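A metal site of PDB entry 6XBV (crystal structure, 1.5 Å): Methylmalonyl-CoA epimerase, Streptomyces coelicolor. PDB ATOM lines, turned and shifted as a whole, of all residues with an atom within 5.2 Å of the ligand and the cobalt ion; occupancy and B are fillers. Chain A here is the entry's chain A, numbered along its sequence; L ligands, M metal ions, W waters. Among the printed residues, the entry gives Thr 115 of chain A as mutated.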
ATOM      1  N   HIS A   7     -13.315  21.746  -4.478  1.00  0.00           N
ATOM      2  CA  HIS A   7     -12.072  21.333  -3.799  1.00  0.00           C
ATOM      3  C   HIS A   7     -11.976  19.819  -3.819  1.00  0.00           C
ATOM      4  O   HIS A   7     -12.962  19.085  -4.004  1.00  0.00           O
ATOM      5  CB  HIS A   7     -11.906  21.900  -2.409  1.00  0.00           C
ATOM      6  CG  HIS A   7     -12.979  21.535  -1.404  1.00  0.00           C
ATOM      7  ND1 HIS A   7     -14.134  22.349  -1.226  1.00  0.00           N
ATOM      8  CD2 HIS A   7     -13.011  20.559  -0.459  1.00  0.00           C
ATOM      9  CE1 HIS A   7     -14.773  21.802  -0.178  1.00  0.00           C
ATOM     10  NE2 HIS A   7     -14.160  20.706   0.312  1.00  0.00           N
ATOM     11  N   ASN A  36     -12.695  23.396  12.455  1.00  0.00           N
ATOM     12  CA  ASN A  36     -14.153  23.201  12.440  1.00  0.00           C
ATOM     13  C   ASN A  36     -14.432  22.176  13.519  1.00  0.00           C
ATOM     14  O   ASN A  36     -14.190  20.982  13.288  1.00  0.00           O
ATOM     15  CB  ASN A  36     -14.686  22.796  11.059  1.00  0.00           C
ATOM     16  CG  ASN A  36     -16.194  22.804  10.993  1.00  0.00           C
ATOM     17  OD1 ASN A  36     -16.831  22.232  11.870  1.00  0.00           O
ATOM     18  ND2 ASN A  36     -16.750  23.325   9.889  1.00  0.00           N
ATOM     19  N   GLN A  39     -17.180  19.411  12.752  1.00  0.00           N
ATOM     20  CA  GLN A  39     -16.733  18.362  11.807  1.00  0.00           C
ATOM     21  C   GLN A  39     -15.529  17.626  12.357  1.00  0.00           C
ATOM     22  O   GLN A  39     -15.285  16.524  11.888  1.00  0.00           O
ATOM     23  CB  GLN A  39     -16.422  18.972  10.428  1.00  0.00           C
ATOM     24  CG  GLN A  39     -17.647  19.493   9.720  1.00  0.00           C
ATOM     25  CD  GLN A  39     -18.599  18.427   9.233  1.00  0.00           C
ATOM     26  OE1 GLN A  39     -18.267  17.226   9.189  1.00  0.00           O
ATOM     27  NE2 GLN A  39     -19.842  18.853   8.978  1.00  0.00           N
ATOM     28  N   VAL A  41     -12.153  18.728  12.402  1.00  0.00           N
ATOM     29  CA  VAL A  41     -10.974  18.891  11.496  1.00  0.00           C
ATOM     30  C   VAL A  41     -10.255  20.211  11.785  1.00  0.00           C
ATOM     31  O   VAL A  41     -10.915  21.241  12.062  1.00  0.00           O
ATOM     32  CB  VAL A  41     -11.355  18.849  10.006  1.00  0.00           C
ATOM     33  CG1 VAL A  41     -11.875  17.475   9.615  1.00  0.00           C
ATOM     34  CG2 VAL A  41     -12.357  19.918   9.600  1.00  0.00           C
ATOM     35  N   GLU A  43      -8.042  22.438   9.147  1.00  0.00           N
ATOM     36  CA  GLU A  43      -7.901  22.387   7.673  1.00  0.00           C
ATOM     37  C   GLU A  43      -7.092  23.527   7.143  1.00  0.00           C
ATOM     38  O   GLU A  43      -6.990  24.647   7.752  1.00  0.00           O
ATOM     39  CB  GLU A  43      -9.254  22.276   7.028  1.00  0.00           C
ATOM     40  CG  GLU A  43     -10.127  23.405   7.376  1.00  0.00           C
ATOM     41  CD  GLU A  43     -11.186  23.710   6.331  1.00  0.00           C
ATOM     42  OE1 GLU A  43     -12.380  23.754   6.714  1.00  0.00           O
ATOM     43  OE2 GLU A  43     -10.800  23.954   5.142  1.00  0.00           O
ATOM     44  N   GLN A  60      -8.112  20.969  -0.132  1.00  0.00           N
ATOM     45  CA  GLN A  60      -8.485  21.110   1.285  1.00  0.00           C
ATOM     46  C   GLN A  60      -7.759  20.016   2.042  1.00  0.00           C
ATOM     47  O   GLN A  60      -8.163  18.833   1.978  1.00  0.00           O
ATOM     48  CB  GLN A  60      -9.992  21.032   1.427  1.00  0.00           C
ATOM     49  CG  GLN A  60     -10.447  21.098   2.870  1.00  0.00           C
ATOM     50  CD  GLN A  60     -11.940  21.043   2.994  1.00  0.00           C
ATOM     51  OE1 GLN A  60     -12.511  20.019   2.695  1.00  0.00           O
ATOM     52  NE2 GLN A  60     -12.532  22.184   3.323  1.00  0.00           N
ATOM     53  N   LEU A  62      -6.802  18.163   5.504  1.00  0.00           N
ATOM     54  CA  LEU A  62      -7.572  17.994   6.752  1.00  0.00           C
ATOM     55  C   LEU A  62      -6.810  17.077   7.669  1.00  0.00           C
ATOM     56  O   LEU A  62      -6.574  15.913   7.322  1.00  0.00           O
ATOM     57  CB  LEU A  62      -8.968  17.411   6.448  1.00  0.00           C
ATOM     58  CG  LEU A  62      -9.802  18.208   5.450  1.00  0.00           C
ATOM     59  CD1 LEU A  62     -10.181  17.278   4.352  1.00  0.00           C
ATOM     60  CD2 LEU A  62     -11.005  18.851   6.083  1.00  0.00           C
ATOM     61  N   ALA A  70     -15.240  11.963  11.499  1.00  0.00           N
ATOM     62  CA  ALA A  70     -15.219  11.379  10.144  1.00  0.00           C
ATOM     63  C   ALA A  70     -13.780  11.143   9.666  1.00  0.00           C
ATOM     64  O   ALA A  70     -13.433  10.074   9.149  1.00  0.00           O
ATOM     65  CB  ALA A  70     -16.012  12.236   9.200  1.00  0.00           C
ATOM     66  N   VAL A  71     -12.935  12.167   9.742  1.00  0.00           N
ATOM     67  CA  VAL A  71     -11.558  12.058   9.210  1.00  0.00           C
ATOM     68  C   VAL A  71     -10.711  11.188  10.136  1.00  0.00           C
ATOM     69  O   VAL A  71      -9.864  10.430   9.597  1.00  0.00           O
ATOM     70  CB  VAL A  71     -10.955  13.449   8.956  1.00  0.00           C
ATOM     71  CG1 VAL A  71      -9.526  13.325   8.534  1.00  0.00           C
ATOM     72  CG2 VAL A  71     -11.769  14.181   7.870  1.00  0.00           C
ATOM     73  N   LYS A  73     -11.610   8.575  11.912  1.00  0.00           N
ATOM     74  CA  LYS A  73     -11.997   7.169  11.656  1.00  0.00           C
ATOM     75  C   LYS A  73     -11.445   6.746  10.299  1.00  0.00           C
ATOM     76  O   LYS A  73     -10.920   5.610  10.118  1.00  0.00           O
ATOM     77  CB  LYS A  73     -13.505   6.973  11.620  1.00  0.00           C
ATOM     78  CG  LYS A  73     -14.220   6.945  12.962  1.00  0.00           C
ATOM     79  CD  LYS A  73     -15.681   6.530  12.807  1.00  0.00           C
ATOM     80  CE  LYS A  73     -15.855   5.299  11.946  1.00  0.00           C
ATOM     81  NZ  LYS A  73     -17.156   4.611  12.183  1.00  0.00           N
ATOM     82  N   TRP A  74     -11.603   7.600   9.304  1.00  0.00           N
ATOM     83  CA  TRP A  74     -11.162   7.263   7.962  1.00  0.00           C
ATOM     84  C   TRP A  74      -9.654   7.044   7.915  1.00  0.00           C
ATOM     85  O   TRP A  74      -9.178   6.098   7.259  1.00  0.00           O
ATOM     86  CB  TRP A  74     -11.674   8.361   7.016  1.00  0.00           C
ATOM     87  CG  TRP A  74     -11.540   7.956   5.609  1.00  0.00           C
ATOM     88  CD1 TRP A  74     -12.446   7.294   4.848  1.00  0.00           C
ATOM     89  CD2 TRP A  74     -10.416   8.211   4.789  1.00  0.00           C
ATOM     90  NE1 TRP A  74     -11.939   7.078   3.618  1.00  0.00           N
ATOM     91  CE2 TRP A  74     -10.702   7.644   3.535  1.00  0.00           C
ATOM     92  CE3 TRP A  74      -9.200   8.850   4.996  1.00  0.00           C
ATOM     93  CZ2 TRP A  74      -9.817   7.714   2.479  1.00  0.00           C
ATOM     94  CZ3 TRP A  74      -8.318   8.914   3.971  1.00  0.00           C
ATOM     95  CH2 TRP A  74      -8.612   8.360   2.742  1.00  0.00           C
ATOM     96  N   LYS A  77      -8.581   3.664   9.372  1.00  0.00           N
ATOM     97  CA  LYS A  77      -8.908   2.526   8.487  1.00  0.00           C
ATOM     98  C   LYS A  77      -8.039   2.544   7.228  1.00  0.00           C
ATOM     99  O   LYS A  77      -7.665   1.467   6.776  1.00  0.00           O
ATOM    100  CB  LYS A  77     -10.371   2.448   8.020  1.00  0.00           C
ATOM    101  CG  LYS A  77     -10.618   1.410   6.908  1.00  0.00           C
ATOM    102  CD  LYS A  77     -11.978   1.409   6.214  1.00  0.00           C
ATOM    103  CE  LYS A  77     -12.092   0.402   5.089  1.00  0.00           C
ATOM    104  NZ  LYS A  77     -11.760   0.970   3.747  1.00  0.00           N
ATOM    105  N   HIS A  83     -10.002  11.913   0.645  1.00  0.00           N
ATOM    106  CA  HIS A  83     -11.151  11.637   1.503  1.00  0.00           C
ATOM    107  C   HIS A  83     -12.481  11.983   0.852  1.00  0.00           C
ATOM    108  O   HIS A  83     -13.448  11.255   1.003  1.00  0.00           O
ATOM    109  CB  HIS A  83     -10.937  12.411   2.804  1.00  0.00           C
ATOM    110  CG  HIS A  83     -12.075  12.296   3.770  1.00  0.00           C
ATOM    111  ND1 HIS A  83     -13.051  13.251   3.920  1.00  0.00           N
ATOM    112  CD2 HIS A  83     -12.452  11.261   4.605  1.00  0.00           C
ATOM    113  CE1 HIS A  83     -13.979  12.807   4.788  1.00  0.00           C
ATOM    114  NE2 HIS A  83     -13.592  11.626   5.239  1.00  0.00           N
ATOM    115  N   HIS A  84     -12.552  13.098   0.097  1.00  0.00           N
ATOM    116  CA  HIS A  84     -13.842  13.503  -0.500  1.00  0.00           C
ATOM    117  C   HIS A  84     -13.595  14.413  -1.687  1.00  0.00           C
ATOM    118  O   HIS A  84     -12.461  14.937  -1.796  1.00  0.00           O
ATOM    119  CB  HIS A  84     -14.822  14.126   0.484  1.00  0.00           C
ATOM    120  CG  HIS A  84     -14.411  15.439   1.059  1.00  0.00           C
ATOM    121  ND1 HIS A  84     -13.692  15.518   2.252  1.00  0.00           N
ATOM    122  CD2 HIS A  84     -14.767  16.719   0.732  1.00  0.00           C
ATOM    123  CE1 HIS A  84     -13.574  16.831   2.566  1.00  0.00           C
ATOM    124  NE2 HIS A  84     -14.235  17.601   1.676  1.00  0.00           N
ATOM    125  N   ALA A  86     -15.582  17.886  -3.671  1.00  0.00           N
ATOM    126  CA  ALA A  86     -16.630  18.882  -3.453  1.00  0.00           C
ATOM    127  C   ALA A  86     -16.955  19.606  -4.759  1.00  0.00           C
ATOM    128  O   ALA A  86     -16.008  20.107  -5.432  1.00  0.00           O
ATOM    129  CB  ALA A  86     -16.187  19.867  -2.398  1.00  0.00           C
ATOM    130  N   LEU A 107     -26.842  13.715   3.659  1.00  0.00           N
ATOM    131  CA  LEU A 107     -26.573  13.439   5.074  1.00  0.00           C
ATOM    132  C   LEU A 107     -27.190  14.541   5.969  1.00  0.00           C
ATOM    133  O   LEU A 107     -27.538  14.187   7.116  1.00  0.00           O
ATOM    134  CB  LEU A 107     -25.071  13.350   5.311  1.00  0.00           C
ATOM    135  CG  LEU A 107     -24.290  12.285   4.593  1.00  0.00           C
ATOM    136  CD1 LEU A 107     -22.907  12.196   5.212  1.00  0.00           C
ATOM    137  CD2 LEU A 107     -24.935  10.927   4.540  1.00  0.00           C
ATOM    138  N   TYR A 108     -27.366  15.765   5.554  1.00  0.00           N
ATOM    139  CA  TYR A 108     -27.911  16.808   6.478  1.00  0.00           C
ATOM    140  C   TYR A 108     -29.315  17.238   6.030  1.00  0.00           C
ATOM    141  O   TYR A 108     -29.555  17.390   4.866  1.00  0.00           O
ATOM    142  CB  TYR A 108     -26.916  17.977   6.549  1.00  0.00           C
ATOM    143  CG  TYR A 108     -25.510  17.595   6.937  1.00  0.00           C
ATOM    144  CD1 TYR A 108     -25.230  16.598   7.818  1.00  0.00           C
ATOM    145  CD2 TYR A 108     -24.425  18.340   6.495  1.00  0.00           C
ATOM    146  CE1 TYR A 108     -23.942  16.236   8.177  1.00  0.00           C
ATOM    147  CE2 TYR A 108     -23.135  17.997   6.816  1.00  0.00           C
ATOM    148  CZ  TYR A 108     -22.862  16.944   7.670  1.00  0.00           C
ATOM    149  OH  TYR A 108     -21.591  16.573   7.960  1.00  0.00           O
ATOM    150  N   ARG A 113     -22.344  24.648   8.402  1.00  0.00           N
ATOM    151  CA  ARG A 113     -21.202  25.586   8.158  1.00  0.00           C
ATOM    152  C   ARG A 113     -19.953  24.817   7.770  1.00  0.00           C
ATOM    153  O   ARG A 113     -19.525  23.851   8.446  1.00  0.00           O
ATOM    154  CB  ARG A 113     -20.841  26.365   9.440  1.00  0.00           C
ATOM    155  CG  ARG A 113     -19.648  27.288   9.246  1.00  0.00           C
ATOM    156  CD  ARG A 113     -19.550  28.481  10.198  1.00  0.00           C
ATOM    157  NE  ARG A 113     -19.318  28.019  11.564  1.00  0.00           N
ATOM    158  CZ  ARG A 113     -18.153  27.608  12.061  1.00  0.00           C
ATOM    159  NH1 ARG A 113     -17.059  27.621  11.324  1.00  0.00           N
ATOM    160  NH2 ARG A 113     -18.090  27.230  13.334  1.00  0.00           N
ATOM    161  N   GLY A 114     -19.326  25.280   6.704  1.00  0.00           N
ATOM    162  CA  GLY A 114     -18.021  24.772   6.276  1.00  0.00           C
ATOM    163  C   GLY A 114     -17.022  25.921   6.212  1.00  0.00           C
ATOM    164  O   GLY A 114     -17.285  27.058   6.747  1.00  0.00           O
ATOM    165  N   THR A 115     -16.002  25.750   5.425  1.00  0.00           N
ATOM    166  CA  THR A 115     -14.800  26.610   5.346  1.00  0.00           C
ATOM    167  C   THR A 115     -15.172  28.042   4.973  1.00  0.00           C
ATOM    168  O   THR A 115     -15.940  28.192   4.019  1.00  0.00           O
ATOM    169  CB  THR A 115     -13.923  26.009   4.248  1.00  0.00           C
ATOM    170  OG1 THR A 115     -13.865  24.623   4.546  1.00  0.00           O
ATOM    171  CG2 THR A 115     -12.566  26.660   4.192  1.00  0.00           C
ATOM    172  N   SER A 118     -18.759  29.018   4.324  1.00  0.00           N
ATOM    173  CA  SER A 118     -19.529  28.327   3.258  1.00  0.00           C
ATOM    174  C   SER A 118     -20.654  27.528   3.929  1.00  0.00           C
ATOM    175  O   SER A 118     -20.607  27.211   5.140  1.00  0.00           O
ATOM    176  CB  SER A 118     -18.639  27.423   2.385  1.00  0.00           C
ATOM    177  OG  SER A 118     -18.001  26.425   3.111  1.00  0.00           O
ATOM    178  N   ILE A 120     -22.569  23.770   3.460  1.00  0.00           N
ATOM    179  CA  ILE A 120     -22.130  22.483   2.830  1.00  0.00           C
ATOM    180  C   ILE A 120     -23.142  21.406   3.151  1.00  0.00           C
ATOM    181  O   ILE A 120     -23.776  21.415   4.229  1.00  0.00           O
ATOM    182  CB  ILE A 120     -20.731  22.058   3.302  1.00  0.00           C
ATOM    183  CG1 ILE A 120     -20.672  21.640   4.777  1.00  0.00           C
ATOM    184  CG2 ILE A 120     -19.727  23.185   2.999  1.00  0.00           C
ATOM    185  CD1 ILE A 120     -19.319  21.132   5.242  1.00  0.00           C
ATOM    186  N   PHE A 122     -23.404  16.776   2.327  1.00  0.00           N
ATOM    187  CA  PHE A 122     -22.687  15.606   1.792  1.00  0.00           C
ATOM    188  C   PHE A 122     -23.676  14.570   1.280  1.00  0.00           C
ATOM    189  O   PHE A 122     -24.806  14.502   1.828  1.00  0.00           O
ATOM    190  CB  PHE A 122     -21.794  14.931   2.809  1.00  0.00           C
ATOM    191  CG  PHE A 122     -20.589  15.732   3.242  1.00  0.00           C
ATOM    192  CD1 PHE A 122     -19.382  15.620   2.580  1.00  0.00           C
ATOM    193  CD2 PHE A 122     -20.700  16.567   4.351  1.00  0.00           C
ATOM    194  CE1 PHE A 122     -18.280  16.387   3.002  1.00  0.00           C
ATOM    195  CE2 PHE A 122     -19.613  17.318   4.749  1.00  0.00           C
ATOM    196  CZ  PHE A 122     -18.414  17.199   4.104  1.00  0.00           C
ATOM    197  N   HIS A 124     -24.021  10.366   0.543  1.00  0.00           N
ATOM    198  CA  HIS A 124     -23.419   9.138   1.088  1.00  0.00           C
ATOM    199  C   HIS A 124     -22.576   8.430   0.022  1.00  0.00           C
ATOM    200  O   HIS A 124     -23.044   8.214  -1.112  1.00  0.00           O
ATOM    201  CB  HIS A 124     -24.555   8.201   1.591  1.00  0.00           C
ATOM    202  CG  HIS A 124     -24.042   7.176   2.522  1.00  0.00           C
ATOM    203  ND1 HIS A 124     -23.137   6.188   2.142  1.00  0.00           N
ATOM    204  CD2 HIS A 124     -24.261   7.022   3.865  1.00  0.00           C
ATOM    205  CE1 HIS A 124     -22.870   5.423   3.243  1.00  0.00           C
ATOM    206  NE2 HIS A 124     -23.503   5.934   4.255  1.00  0.00           N
ATOM    207  N   PRO A 125     -21.301   8.068   0.341  1.00  0.00           N
ATOM    208  CA  PRO A 125     -20.463   7.435  -0.648  1.00  0.00           C
ATOM    209  C   PRO A 125     -20.991   6.147  -1.215  1.00  0.00           C
ATOM    210  O   PRO A 125     -20.736   5.824  -2.385  1.00  0.00           O
ATOM    211  CB  PRO A 125     -19.146   7.239   0.096  1.00  0.00           C
ATOM    212  CG  PRO A 125     -19.526   7.214   1.567  1.00  0.00           C
ATOM    213  CD  PRO A 125     -20.656   8.225   1.641  1.00  0.00           C
ATOM    214  N   LYS A 126     -21.778   5.409  -0.401  1.00  0.00           N
ATOM    215  CA  LYS A 126     -22.293   4.153  -0.973  1.00  0.00           C
ATOM    216  C   LYS A 126     -23.371   4.398  -2.003  1.00  0.00           C
ATOM    217  O   LYS A 126     -23.705   3.416  -2.744  1.00  0.00           O
ATOM    218  CB  LYS A 126     -22.867   3.328   0.195  1.00  0.00           C
ATOM    219  CG  LYS A 126     -21.807   2.820   1.142  1.00  0.00           C
ATOM    220  CD  LYS A 126     -20.839   1.851   0.541  1.00  0.00           C
ATOM    221  CE  LYS A 126     -21.545   0.572   0.137  1.00  0.00           C
ATOM    222  NZ  LYS A 126     -22.448   0.036   1.197  1.00  0.00           N
ATOM    223  N   GLY A 130     -18.805   4.983  -4.357  1.00  0.00           N
ATOM    224  CA  GLY A 130     -17.640   4.965  -3.473  1.00  0.00           C
ATOM    225  C   GLY A 130     -16.994   6.319  -3.213  1.00  0.00           C
ATOM    226  O   GLY A 130     -15.927   6.314  -2.631  1.00  0.00           O
ATOM    227  N   VAL A 131     -17.615   7.402  -3.722  1.00  0.00           N
ATOM    228  CA  VAL A 131     -16.995   8.752  -3.579  1.00  0.00           C
ATOM    229  C   VAL A 131     -17.824   9.592  -2.614  1.00  0.00           C
ATOM    230  O   VAL A 131     -19.006   9.891  -2.875  1.00  0.00           O
ATOM    231  CB  VAL A 131     -16.869   9.453  -4.950  1.00  0.00           C
ATOM    232  CG1 VAL A 131     -16.299  10.865  -4.732  1.00  0.00           C
ATOM    233  CG2 VAL A 131     -16.008   8.632  -5.858  1.00  0.00           C
ATOM    234  N   LEU A 132     -17.244   9.935  -1.449  1.00  0.00           N
ATOM    235  CA  LEU A 132     -17.901  10.896  -0.548  1.00  0.00           C
ATOM    236  C   LEU A 132     -17.960  12.227  -1.300  1.00  0.00           C
ATOM    237  O   LEU A 132     -16.888  12.754  -1.619  1.00  0.00           O
ATOM    238  CB  LEU A 132     -17.197  10.960   0.807  1.00  0.00           C
ATOM    239  CG  LEU A 132     -17.747  12.017   1.770  1.00  0.00           C
ATOM    240  CD1 LEU A 132     -19.207  11.807   2.202  1.00  0.00           C
ATOM    241  CD2 LEU A 132     -16.861  12.031   3.005  1.00  0.00           C
ATOM    242  N   GLU A 134     -19.280  16.164  -1.566  1.00  0.00           N
ATOM    243  CA  GLU A 134     -19.735  17.412  -0.902  1.00  0.00           C
ATOM    244  C   GLU A 134     -20.349  18.348  -1.912  1.00  0.00           C
ATOM    245  O   GLU A 134     -19.830  18.460  -3.055  1.00  0.00           O
ATOM    246  CB  GLU A 134     -18.553  18.052  -0.185  1.00  0.00           C
ATOM    247  CG  GLU A 134     -18.879  19.270   0.660  1.00  0.00           C
ATOM    248  CD  GLU A 134     -17.672  19.972   1.249  1.00  0.00           C
ATOM    249  OE1 GLU A 134     -16.683  19.314   1.475  1.00  0.00           O
ATOM    250  OE2 GLU A 134     -17.719  21.293   1.208  1.00  0.00           O
HETATM  251  N1  LIG L   1     -15.129   7.812   1.113  1.00  0.00           N
HETATM  252  C1  LIG L   1     -15.641   6.640   0.661  1.00  0.00           C
HETATM  253  N2  LIG L   1     -16.282   5.770   1.374  1.00  0.00           N
HETATM  254  C2  LIG L   1     -16.336   5.983   2.686  1.00  0.00           C
HETATM  255  C3  LIG L   1     -15.815   7.178   3.293  1.00  0.00           C
HETATM  256  C4  LIG L   1     -15.115   8.143   2.434  1.00  0.00           C
HETATM  257  N3  LIG L   1     -14.606   9.299   2.902  1.00  0.00           N
HETATM  258  N4  LIG L   1     -16.004   7.189   4.649  1.00  0.00           N
HETATM  259  C5  LIG L   1     -16.680   5.990   4.837  1.00  0.00           C
HETATM  260  N5  LIG L   1     -16.877   5.305   3.732  1.00  0.00           N
HETATM  261  C6  LIG L   1     -17.555   3.968   3.594  1.00  0.00           C
HETATM  262  C7  LIG L   1     -16.913   2.930   4.550  1.00  0.00           C
HETATM  263  O1  LIG L   1     -15.763   2.345   4.001  1.00  0.00           O
HETATM  264  C8  LIG L   1     -18.041   1.933   4.775  1.00  0.00           C
HETATM  265  O2  LIG L   1     -18.066   1.176   3.584  1.00  0.00           O
HETATM  266  C9  LIG L   1     -19.238   2.854   4.818  1.00  0.00           C
HETATM  267  O3  LIG L   1     -18.835   4.095   4.139  1.00  0.00           O
HETATM  268  C10 LIG L   1     -19.595   3.267   6.193  1.00  0.00           C
HETATM  269  O4  LIG L   1     -18.378   3.564   6.860  1.00  0.00           O
HETATM  270  O5  LIG L   1     -16.598  -0.728   4.446  1.00  0.00           O
HETATM  271  P1  LIG L   1     -17.913  -0.461   3.768  1.00  0.00           P
HETATM  272  O6  LIG L   1     -19.022  -0.778   4.777  1.00  0.00           O
HETATM  273  O7  LIG L   1     -17.991  -0.921   2.320  1.00  0.00           O
HETATM  274  P2  LIG L   1     -18.194   3.925   8.415  1.00  0.00           P
HETATM  275  O8  LIG L   1     -19.068   2.954   9.152  1.00  0.00           O
HETATM  276  O9  LIG L   1     -16.689   3.752   8.607  1.00  0.00           O
HETATM  277  O10 LIG L   1     -18.431   5.400   8.964  1.00  0.00           O
HETATM  278  P3  LIG L   1     -19.894   6.036   8.915  1.00  0.00           P
HETATM  279  O11 LIG L   1     -20.855   5.177   8.164  1.00  0.00           O
HETATM  280  O12 LIG L   1     -20.513   6.426  10.242  1.00  0.00           O
HETATM  281  O13 LIG L   1     -19.540   7.443   8.193  1.00  0.00           O
HETATM  282  C11 LIG L   1     -19.538   7.534   6.779  1.00  0.00           C
HETATM  283  C12 LIG L   1     -19.948   8.968   6.529  1.00  0.00           C
HETATM  284  C13 LIG L   1     -20.514   9.316   5.197  1.00  0.00           C
HETATM  285  C14 LIG L   1     -21.341   8.921   7.163  1.00  0.00           C
HETATM  286  C15 LIG L   1     -19.440   9.978   7.459  1.00  0.00           C
HETATM  287  O14 LIG L   1     -18.052   9.948   7.407  1.00  0.00           O
HETATM  288  C16 LIG L   1     -19.780  11.370   7.209  1.00  0.00           C
HETATM  289  O15 LIG L   1     -20.740  11.810   7.798  1.00  0.00           O
HETATM  290  N6  LIG L   1     -19.139  12.208   6.354  1.00  0.00           N
HETATM  291  C17 LIG L   1     -19.506  13.604   6.187  1.00  0.00           C
HETATM  292  C18 LIG L   1     -18.748  14.603   7.064  1.00  0.00           C
HETATM  293  C19 LIG L   1     -17.272  14.712   6.783  1.00  0.00           C
HETATM  294  O16 LIG L   1     -16.727  13.853   6.053  1.00  0.00           O
HETATM  295  N7  LIG L   1     -16.598  15.607   7.465  1.00  0.00           N
HETATM  296  C20 LIG L   1     -15.178  15.831   7.336  1.00  0.00           C
HETATM  297  C21 LIG L   1     -14.947  16.865   6.184  1.00  0.00           C
HETATM  298  S1  LIG L   1     -15.320  18.544   6.786  1.00  0.00           S
HETATM  299  C22 LIG L   1     -15.244  19.506   5.364  1.00  0.00           C
HETATM  300  O17 LIG L   1     -15.019  19.039   4.249  1.00  0.00           O
HETATM  301  C23 LIG L   1     -15.546  20.891   5.511  1.00  0.00           C
HETATM  302  C24 LIG L   1     -15.608  21.516   6.901  1.00  0.00           C
HETATM  303  N8  LIG L   1     -15.607  21.764   4.402  1.00  0.00           N
HETATM  304  O18 LIG L   1     -15.406  21.480   3.168  1.00  0.00           O
HETATM  305  O19 LIG L   1     -15.971  22.977   4.717  1.00  0.00           O
HETATM  306 CO    CO M   1     -14.705  19.678   2.161  1.00  0.00          CO
HETATM  307  O   HOH W   1     -15.468   9.552   6.093  1.00  0.00           O
HETATM  308  O   HOH W   2     -16.488  24.110   2.017  1.00  0.00           O
HETATM  309  O   HOH W   3     -14.416   9.373  -1.080  1.00  0.00           O
HETATM  310  O   HOH W   4     -21.448  14.083   9.128  1.00  0.00           O
HETATM  311  O   HOH W   5     -14.382   5.381   7.767  1.00  0.00           O
HETATM  312  O   HOH W   6     -24.489   7.667   7.869  1.00  0.00           O
HETATM  313  O   HOH W   7     -22.655   2.505   4.982  1.00  0.00           O
HETATM  314  O   HOH W   8     -15.362   8.167   8.644  1.00  0.00           O
HETATM  315  O   HOH W   9     -19.134  -0.887  -0.885  1.00  0.00           O
HETATM  316  O   HOH W  10     -21.652   8.624  11.221  1.00  0.00           O
HETATM  317  O   HOH W  11     -23.132   5.145   7.040  1.00  0.00           O
HETATM  318  O   HOH W  12     -13.623   3.868   5.582  1.00  0.00           O
HETATM  319  O   HOH W  13     -19.376  -0.099   7.476  1.00  0.00           O
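The backbone NH (N) of Thr 115 sits at hydrogen-bond distance from an oxygen (O19) of the ligand, at 2.9 Å.
O19 of the ligand lies within hydrogen-bond range of OG1 of Thr 115 (2.7 Å).
The side-chain amide oxygen (OE1) of Gln 39 lies within hydrogen-bond range of a nitrogen (N7) of the ligand (2.9 Å).
N3 of the ligand sits at hydrogen-bond distance from O of His 83, 3.0 Å away.
NE2 of His 83 lies close to N3 of the ligand (3.5 Å).
NZ of Lys 73 is in salt-bridge range of O9 of the ligand, 3.7 Å away.
Merely in contact with the ligand: Gly 114, Gly 130, Leu 107, Pro 125, Trp 74, Leu 132, Ala 70, Tyr 108, Phe 122, Asn 36, Ile 120, Val 71 and Glu 43.
Hydrophobic or aromatic side chains within 4 Å of the ligand: His 7, Ala 70, Val 71, Trp 74, His 83, His 84, Leu 107, Ile 120, Phe 122, Pro 125 and Leu 132.
Within 4 Å of the ligand: His 7, Asn 36, Gln 39, Glu 43, Gln 60, Ala 70, Val 71, Lys 73, Trp 74, His 83, His 84, Leu 107, Tyr 108, Gly 114, Thr 115, Ile 120, Phe 122, Pro 125, Gly 130, Leu 132 and Glu 134.
The nearest printed residue that does not touch the ligand is Lys 126 (4.2 Å).
Four residues have an atom within 4 Å of the cobalt ion: His 7, Gln 60, His 84 and Glu 134.
The side-chain carboxylate (OE1) of Glu 134 binds the cobalt ion, 2.1 Å away.
The cobalt ion is bound by O18 of the ligand, at 2.2 Å.
NE2 of His 84 binds the cobalt ion (2.2 Å).
NE2 of His 7 binds the cobalt ion (2.2 Å).
O17 of the ligand binds the cobalt ion (2.2 Å).
The cobalt ion is bound by the side-chain amide oxygen (OE1) of Gln 60 (2.3 Å).
Water W11 lies within hydrogen-bond range of an oxygen (O11) of the ligand and a ring nitrogen (NE2) of His 124.
Water W4 lies within hydrogen-bond range of an oxygen (O15) of the ligand (2.7 Å) and the side-chain hydroxyl (OH) of Tyr 108 (2.8 Å).
Water W3 lies within hydrogen-bond range of a nitrogen (N1) of the ligand (2.8 Å), the backbone NH of Leu 132 (2.9 Å) and the backbone carbonyl oxygen of His 83 (3.0 Å).
Water W1 bridges N4 of the ligand (2.8 Å) and NE2 of His 83 (2.9 Å).
Water W2 lies within hydrogen-bond range of an oxygen (O19) of the ligand (3.0 Å), the side-chain hydroxyl (OG) of Ser 118 (3.0 Å) and the side-chain carboxylate (OE2) of Glu 134 (3.2 Å).
Water W8 bridges the backbone carbonyl oxygen of Ala 70 (2.8 Å) and an oxygen (O14) of the ligand (3.5 Å).
A ring nitrogen (ND1) of His 83 lies within hydrogen-bond range of a ring nitrogen (ND1) of His 84.
The backbone NH of Ala 86 is in hydrogen-bond range of the backbone carbonyl oxygen of His 7, 2.9 Å away.
The side-chain amide nitrogen (NE2) of Gln 60 is in hydrogen-bond range of the side-chain hydroxyl (OG1) of Thr 115 (3.0 Å).
The side-chain carboxylate (OE1) of Glu 43 lies within hydrogen-bond range of the side-chain hydroxyl (OG1) of Thr 115 (2.8 Å).
The backbone carbonyl oxygen (O) of Thr 115 sits at hydrogen-bond distance from the side-chain hydroxyl (OG) of Ser 118, at 2.9 Å.
The side-chain amide nitrogen (NE2) of Gln 39 sits at hydrogen-bond distance from the side-chain hydroxyl (OH) of Tyr 108 (3.0 Å).
The backbone carbonyl oxygen (O) of Phe 122 lies within hydrogen-bond range of the backbone NH (N) of Leu 107 (2.8 Å).
The backbone carbonyl oxygen of Arg 113 lies within hydrogen-bond range of the side-chain amide nitrogen of Asn 36, at 3.2 Å.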
